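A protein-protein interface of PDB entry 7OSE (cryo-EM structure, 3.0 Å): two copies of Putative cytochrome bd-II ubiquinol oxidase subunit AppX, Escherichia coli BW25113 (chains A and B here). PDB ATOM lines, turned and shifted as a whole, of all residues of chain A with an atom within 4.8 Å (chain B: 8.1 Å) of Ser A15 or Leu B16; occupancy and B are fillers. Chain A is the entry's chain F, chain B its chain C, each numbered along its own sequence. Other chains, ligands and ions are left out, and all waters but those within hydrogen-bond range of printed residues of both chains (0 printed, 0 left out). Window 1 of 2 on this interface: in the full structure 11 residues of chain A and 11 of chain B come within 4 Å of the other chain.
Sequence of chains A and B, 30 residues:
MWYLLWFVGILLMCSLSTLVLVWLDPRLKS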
ATOM      1  N   LEU A  11      -6.317   0.328  30.184  1.00  0.00           N
ATOM      2  CA  LEU A  11      -6.444   0.678  28.772  1.00  0.00           C
ATOM      3  C   LEU A  11      -5.655  -0.290  27.894  1.00  0.00           C
ATOM      4  O   LEU A  11      -6.111  -0.675  26.810  1.00  0.00           O
ATOM      5  CB  LEU A  11      -5.993   2.117  28.538  1.00  0.00           C
ATOM      6  CG  LEU A  11      -6.969   3.206  28.977  1.00  0.00           C
ATOM      7  CD1 LEU A  11      -6.454   4.573  28.568  1.00  0.00           C
ATOM      8  CD2 LEU A  11      -8.342   2.951  28.384  1.00  0.00           C
ATOM      9  N   LEU A  12      -4.471  -0.702  28.354  1.00  0.00           N
ATOM     10  CA  LEU A  12      -3.674  -1.674  27.614  1.00  0.00           C
ATOM     11  C   LEU A  12      -4.394  -3.009  27.495  1.00  0.00           C
ATOM     12  O   LEU A  12      -4.398  -3.622  26.424  1.00  0.00           O
ATOM     13  CB  LEU A  12      -2.315  -1.850  28.293  1.00  0.00           C
ATOM     14  CG  LEU A  12      -1.220  -2.677  27.613  1.00  0.00           C
ATOM     15  CD1 LEU A  12       0.124  -2.091  27.959  1.00  0.00           C
ATOM     16  CD2 LEU A  12      -1.259  -4.134  28.052  1.00  0.00           C
ATOM     17  N   MET A  13      -4.988  -3.485  28.589  1.00  0.00           N
ATOM     18  CA  MET A  13      -5.720  -4.747  28.548  1.00  0.00           C
ATOM     19  C   MET A  13      -6.901  -4.655  27.595  1.00  0.00           C
ATOM     20  O   MET A  13      -7.167  -5.586  26.825  1.00  0.00           O
ATOM     21  CB  MET A  13      -6.195  -5.128  29.949  1.00  0.00           C
ATOM     22  CG  MET A  13      -5.080  -5.446  30.925  1.00  0.00           C
ATOM     23  SD  MET A  13      -5.632  -5.392  32.641  1.00  0.00           S
ATOM     24  CE  MET A  13      -6.975  -6.573  32.601  1.00  0.00           C
ATOM     25  N   CYS A  14      -7.615  -3.528  27.629  1.00  0.00           N
ATOM     26  CA  CYS A  14      -8.739  -3.330  26.725  1.00  0.00           C
ATOM     27  C   CYS A  14      -8.290  -3.378  25.269  1.00  0.00           C
ATOM     28  O   CYS A  14      -8.889  -4.075  24.438  1.00  0.00           O
ATOM     29  CB  CYS A  14      -9.416  -1.997  27.041  1.00  0.00           C
ATOM     30  SG  CYS A  14     -10.276  -1.975  28.630  1.00  0.00           S
ATOM     31  N   SER A  15      -7.217  -2.655  24.948  1.00  0.00           N
ATOM     32  CA  SER A  15      -6.746  -2.614  23.569  1.00  0.00           C
ATOM     33  C   SER A  15      -6.200  -3.967  23.127  1.00  0.00           C
ATOM     34  O   SER A  15      -6.389  -4.367  21.973  1.00  0.00           O
ATOM     35  CB  SER A  15      -5.695  -1.521  23.415  1.00  0.00           C
ATOM     36  OG  SER A  15      -6.234  -0.256  23.752  1.00  0.00           O
ATOM     37  N   LEU A  16      -5.518  -4.682  24.024  1.00  0.00           N
ATOM     38  CA  LEU A  16      -5.017  -6.011  23.687  1.00  0.00           C
ATOM     39  C   LEU A  16      -6.158  -6.975  23.397  1.00  0.00           C
ATOM     40  O   LEU A  16      -6.096  -7.745  22.435  1.00  0.00           O
ATOM     41  CB  LEU A  16      -4.142  -6.549  24.819  1.00  0.00           C
ATOM     42  CG  LEU A  16      -2.628  -6.436  24.648  1.00  0.00           C
ATOM     43  CD1 LEU A  16      -2.173  -7.239  23.443  1.00  0.00           C
ATOM     44  CD2 LEU A  16      -2.202  -4.987  24.519  1.00  0.00           C
ATOM     45  N   SER A  17      -7.208  -6.949  24.222  1.00  0.00           N
ATOM     46  CA  SER A  17      -8.357  -7.810  23.964  1.00  0.00           C
ATOM     47  C   SER A  17      -9.015  -7.458  22.639  1.00  0.00           C
ATOM     48  O   SER A  17      -9.375  -8.349  21.857  1.00  0.00           O
ATOM     49  CB  SER A  17      -9.359  -7.704  25.111  1.00  0.00           C
ATOM     50  OG  SER A  17      -8.765  -8.079  26.340  1.00  0.00           O
ATOM     51  N   THR A  18      -9.166  -6.161  22.360  1.00  0.00           N
ATOM     52  CA  THR A  18      -9.768  -5.743  21.098  1.00  0.00           C
ATOM     53  C   THR A  18      -8.940  -6.221  19.910  1.00  0.00           C
ATOM     54  O   THR A  18      -9.483  -6.738  18.929  1.00  0.00           O
ATOM     55  CB  THR A  18      -9.922  -4.223  21.068  1.00  0.00           C
ATOM     56  OG1 THR A  18     -10.516  -3.777  22.291  1.00  0.00           O
ATOM     57  CG2 THR A  18     -10.809  -3.808  19.910  1.00  0.00           C
ATOM     58  N   LEU A  19      -7.616  -6.062  19.987  1.00  0.00           N
ATOM     59  CA  LEU A  19      -6.750  -6.487  18.891  1.00  0.00           C
ATOM     60  C   LEU A  19      -6.793  -7.995  18.697  1.00  0.00           C
ATOM     61  O   LEU A  19      -6.839  -8.482  17.561  1.00  0.00           O
ATOM     62  CB  LEU A  19      -5.317  -6.026  19.144  1.00  0.00           C
ATOM     63  CG  LEU A  19      -5.003  -4.588  18.749  1.00  0.00           C
ATOM     64  CD1 LEU A  19      -3.536  -4.279  18.989  1.00  0.00           C
ATOM     65  CD2 LEU A  19      -5.369  -4.371  17.295  1.00  0.00           C
ATOM     66  N   GLY B   9       2.977   1.635  29.098  1.00  0.00           N
ATOM     67  CA  GLY B   9       2.597   2.772  28.279  1.00  0.00           C
ATOM     68  C   GLY B   9       2.953   2.605  26.816  1.00  0.00           C
ATOM     69  O   GLY B   9       2.172   2.973  25.936  1.00  0.00           O
ATOM     70  N   ILE B  10       4.137   2.064  26.527  1.00  0.00           N
ATOM     71  CA  ILE B  10       4.522   1.876  25.134  1.00  0.00           C
ATOM     72  C   ILE B  10       3.677   0.785  24.493  1.00  0.00           C
ATOM     73  O   ILE B  10       3.265   0.908  23.332  1.00  0.00           O
ATOM     74  CB  ILE B  10       6.033   1.594  25.001  1.00  0.00           C
ATOM     75  CG1 ILE B  10       6.424   1.504  23.526  1.00  0.00           C
ATOM     76  CG2 ILE B  10       6.427   0.314  25.702  1.00  0.00           C
ATOM     77  CD1 ILE B  10       5.957   2.674  22.693  1.00  0.00           C
ATOM     78  N   LEU B  11       3.375  -0.286  25.234  1.00  0.00           N
ATOM     79  CA  LEU B  11       2.466  -1.287  24.684  1.00  0.00           C
ATOM     80  C   LEU B  11       1.083  -0.691  24.436  1.00  0.00           C
ATOM     81  O   LEU B  11       0.434  -0.999  23.428  1.00  0.00           O
ATOM     82  CB  LEU B  11       2.381  -2.497  25.610  1.00  0.00           C
ATOM     83  CG  LEU B  11       3.573  -3.450  25.579  1.00  0.00           C
ATOM     84  CD1 LEU B  11       3.298  -4.667  26.442  1.00  0.00           C
ATOM     85  CD2 LEU B  11       3.879  -3.863  24.151  1.00  0.00           C
ATOM     86  N   LEU B  12       0.621   0.173  25.342  1.00  0.00           N
ATOM     87  CA  LEU B  12      -0.664   0.839  25.160  1.00  0.00           C
ATOM     88  C   LEU B  12      -0.660   1.726  23.924  1.00  0.00           C
ATOM     89  O   LEU B  12      -1.627   1.730  23.157  1.00  0.00           O
ATOM     90  CB  LEU B  12      -1.004   1.654  26.409  1.00  0.00           C
ATOM     91  CG  LEU B  12      -2.384   2.302  26.549  1.00  0.00           C
ATOM     92  CD1 LEU B  12      -2.777   2.312  28.002  1.00  0.00           C
ATOM     93  CD2 LEU B  12      -2.395   3.729  26.019  1.00  0.00           C
ATOM     94  N   MET B  13       0.408   2.500  23.727  1.00  0.00           N
ATOM     95  CA  MET B  13       0.495   3.358  22.550  1.00  0.00           C
ATOM     96  C   MET B  13       0.500   2.530  21.276  1.00  0.00           C
ATOM     97  O   MET B  13      -0.161   2.879  20.290  1.00  0.00           O
ATOM     98  CB  MET B  13       1.750   4.228  22.623  1.00  0.00           C
ATOM     99  CG  MET B  13       1.746   5.241  23.750  1.00  0.00           C
ATOM    100  SD  MET B  13       3.395   5.874  24.111  1.00  0.00           S
ATOM    101  CE  MET B  13       3.871   6.512  22.509  1.00  0.00           C
ATOM    102  N   CYS B  14       1.237   1.417  21.284  1.00  0.00           N
ATOM    103  CA  CYS B  14       1.271   0.535  20.125  1.00  0.00           C
ATOM    104  C   CYS B  14      -0.117  -0.005  19.803  1.00  0.00           C
ATOM    105  O   CYS B  14      -0.566   0.035  18.650  1.00  0.00           O
ATOM    106  CB  CYS B  14       2.252  -0.606  20.385  1.00  0.00           C
ATOM    107  SG  CYS B  14       3.981  -0.085  20.440  1.00  0.00           S
ATOM    108  N   SER B  15      -0.821  -0.497  20.823  1.00  0.00           N
ATOM    109  CA  SER B  15      -2.142  -1.071  20.594  1.00  0.00           C
ATOM    110  C   SER B  15      -3.145  -0.005  20.170  1.00  0.00           C
ATOM    111  O   SER B  15      -4.011  -0.264  19.327  1.00  0.00           O
ATOM    112  CB  SER B  15      -2.612  -1.800  21.847  1.00  0.00           C
ATOM    113  OG  SER B  15      -1.715  -2.840  22.189  1.00  0.00           O
ATOM    114  N   LEU B  16      -3.051   1.197  20.743  1.00  0.00           N
ATOM    115  CA  LEU B  16      -3.941   2.282  20.342  1.00  0.00           C
ATOM    116  C   LEU B  16      -3.722   2.668  18.888  1.00  0.00           C
ATOM    117  O   LEU B  16      -4.686   2.874  18.143  1.00  0.00           O
ATOM    118  CB  LEU B  16      -3.739   3.495  21.249  1.00  0.00           C
ATOM    119  CG  LEU B  16      -4.745   3.700  22.381  1.00  0.00           C
ATOM    120  CD1 LEU B  16      -6.137   3.916  21.814  1.00  0.00           C
ATOM    121  CD2 LEU B  16      -4.734   2.525  23.339  1.00  0.00           C
ATOM    122  N   SER B  17      -2.460   2.775  18.464  1.00  0.00           N
ATOM    123  CA  SER B  17      -2.187   3.089  17.066  1.00  0.00           C
ATOM    124  C   SER B  17      -2.713   1.994  16.149  1.00  0.00           C
ATOM    125  O   SER B  17      -3.317   2.282  15.106  1.00  0.00           O
ATOM    126  CB  SER B  17      -0.688   3.295  16.857  1.00  0.00           C
ATOM    127  OG  SER B  17      -0.203   4.346  17.673  1.00  0.00           O
ATOM    128  N   THR B  18      -2.508   0.731  16.530  1.00  0.00           N
ATOM    129  CA  THR B  18      -3.003  -0.373  15.716  1.00  0.00           C
ATOM    130  C   THR B  18      -4.522  -0.329  15.595  1.00  0.00           C
ATOM    131  O   THR B  18      -5.074  -0.498  14.502  1.00  0.00           O
ATOM    132  CB  THR B  18      -2.551  -1.707  16.309  1.00  0.00           C
ATOM    133  OG1 THR B  18      -1.152  -1.649  16.609  1.00  0.00           O
ATOM    134  CG2 THR B  18      -2.797  -2.832  15.322  1.00  0.00           C
ATOM    135  N   LEU B  19      -5.216  -0.093  16.711  1.00  0.00           N
ATOM    136  CA  LEU B  19      -6.675  -0.040  16.686  1.00  0.00           C
ATOM    137  C   LEU B  19      -7.177   1.128  15.849  1.00  0.00           C
ATOM    138  O   LEU B  19      -8.136   0.984  15.081  1.00  0.00           O
ATOM    139  CB  LEU B  19      -7.223   0.054  18.107  1.00  0.00           C
ATOM    140  CG  LEU B  19      -7.349  -1.267  18.858  1.00  0.00           C
ATOM    141  CD1 LEU B  19      -7.966  -1.043  20.227  1.00  0.00           C
ATOM    142  CD2 LEU B  19      -8.181  -2.235  18.042  1.00  0.00           C
ATOM    143  N   VAL B  20      -6.550   2.297  15.992  1.00  0.00           N
ATOM    144  CA  VAL B  20      -6.974   3.459  15.220  1.00  0.00           C
ATOM    145  C   VAL B  20      -6.787   3.201  13.733  1.00  0.00           C
ATOM    146  O   VAL B  20      -7.640   3.561  12.915  1.00  0.00           O
ATOM    147  CB  VAL B  20      -6.217   4.717  15.682  1.00  0.00           C
ATOM    148  CG1 VAL B  20      -6.400   5.844  14.684  1.00  0.00           C
ATOM    149  CG2 VAL B  20      -6.705   5.143  17.054  1.00  0.00           C
ATOM    150  N   LEU B  21      -5.678   2.562  13.357  1.00  0.00           N
ATOM    151  CA  LEU B  21      -5.459   2.273  11.943  1.00  0.00           C
ATOM    152  C   LEU B  21      -6.430   1.218  11.426  1.00  0.00           C
ATOM    153  O   LEU B  21      -6.880   1.297  10.277  1.00  0.00           O
ATOM    154  CB  LEU B  21      -4.018   1.841  11.709  1.00  0.00           C
ATOM    155  CG  LEU B  21      -3.147   2.954  11.134  1.00  0.00           C
ATOM    156  CD1 LEU B  21      -3.546   3.240   9.698  1.00  0.00           C
ATOM    157  CD2 LEU B  21      -3.256   4.216  11.975  1.00  0.00           C
ATOM    158  N   VAL B  22      -6.761   0.220  12.249  1.00  0.00           N
ATOM    159  CA  VAL B  22      -7.735  -0.782  11.828  1.00  0.00           C
ATOM    160  C   VAL B  22      -9.095  -0.136  11.599  1.00  0.00           C
ATOM    161  O   VAL B  22      -9.781  -0.427  10.612  1.00  0.00           O
ATOM    162  CB  VAL B  22      -7.816  -1.925  12.857  1.00  0.00           C
ATOM    163  CG1 VAL B  22      -8.986  -2.838  12.541  1.00  0.00           C
ATOM    164  CG2 VAL B  22      -6.527  -2.720  12.865  1.00  0.00           C
ATOM    165  N   TRP B  23      -9.504   0.754  12.505  1.00  0.00           N
ATOM    166  CA  TRP B  23     -10.787   1.432  12.343  1.00  0.00           C
ATOM    167  C   TRP B  23     -10.778   2.375  11.146  1.00  0.00           C
ATOM    168  O   TRP B  23     -11.769   2.463  10.411  1.00  0.00           O
ATOM    169  CB  TRP B  23     -11.141   2.195  13.618  1.00  0.00           C
ATOM    170  CG  TRP B  23     -12.245   3.188  13.429  1.00  0.00           C
ATOM    171  CD1 TRP B  23     -13.579   2.925  13.351  1.00  0.00           C
ATOM    172  CD2 TRP B  23     -12.108   4.607  13.296  1.00  0.00           C
ATOM    173  NE1 TRP B  23     -14.282   4.089  13.176  1.00  0.00           N
ATOM    174  CE2 TRP B  23     -13.401   5.138  13.139  1.00  0.00           C
ATOM    175  CE3 TRP B  23     -11.016   5.480  13.294  1.00  0.00           C
ATOM    176  CZ2 TRP B  23     -13.635   6.502  12.982  1.00  0.00           C
ATOM    177  CZ3 TRP B  23     -11.250   6.833  13.138  1.00  0.00           C
ATOM    178  CH2 TRP B  23     -12.548   7.330  12.983  1.00  0.00           C
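The backbone carbonyl oxygen (O) of Cys A14 is in hydrogen-bond range of the side-chain hydroxyl (OG1) of Thr A18 (2.7 Å). The side-chain hydroxyl of Ser B15 is in hydrogen-bond range of the backbone carbonyl oxygen of Leu B11, at 3.1 Å. The backbone carbonyl oxygen of Leu A11 is in hydrogen-bond range of the side-chain hydroxyl of Ser A15 (3.1 Å). The backbone carbonyl oxygen (O) of Cys B14 sits at hydrogen-bond distance from the side-chain hydroxyl (OG1) of Thr B18, at 2.7 Å.
Among the printed residues, pairs that only touch across the chains: Ser A15 with Leu B16 (3.2 Å), Leu A16 with Ser B15 (3.2 Å), Leu A11 with Leu B12 (3.3 Å), Leu A12 with Leu B11 (3.3 Å), Ser A15 with Ser B15 (3.5 Å), Leu A12 with Leu B12 (3.5 Å), Thr A18 with Leu B19 (3.6 Å), Leu A19 with Thr B18 (3.6 Å), Leu A19 with Leu B19 (3.6 Å), Leu A19 with Ser B15 (3.8 Å) and Ser A15 with Leu B19 (3.9 Å).
Of the printed residues of chain B, Leu A11 touches Leu B12. Ser A15 touches three residues of chain B. Of the printed residues of chain A, Leu B11 touches Leu A12 (3.3 Å). Of the printed residues of chain A, Leu B12 touches Leu A11 (3.3 Å) and Leu A12 (3.5 Å). Of chain A, only Ser A15 (3.2 Å) comes within 4 Å of Leu B16. Printed residues of chain A within 4 Å of Thr B18: Leu A19. Val B22 touches none of the printed residues of chain A. Trp B23 touches none of the printed residues of chain A. The nearest printed residue of chain A that does not touch Leu B16 is Leu A11 (4.9 Å). The nearest printed residue of chain A that does not touch Leu B12 is Ser A15 (5.1 Å).
Hydrophobic or aromatic side chains of chain A within 4 Å of the printed part of chain B: Leu A11, Leu A12, Leu A16 and Leu A19. Along chain A the printed residues that touch a printed residue of chain B span positions 11 to 19.
Leu B12 touches its own counterpart, Leu A12. Ser A15 touches Leu B19, and with the chains exchanged Leu A19 touches Ser B15. Thr A18 touches Leu B19, and with the chains exchanged Leu A19 touches Thr B18. Leu A19 touches its own counterpart, Leu B19. 9 positions are printed for both chains. Of the 11 pairs that touch across the chains among the printed residues, 11 have their exchanged pair printed and touching as well.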
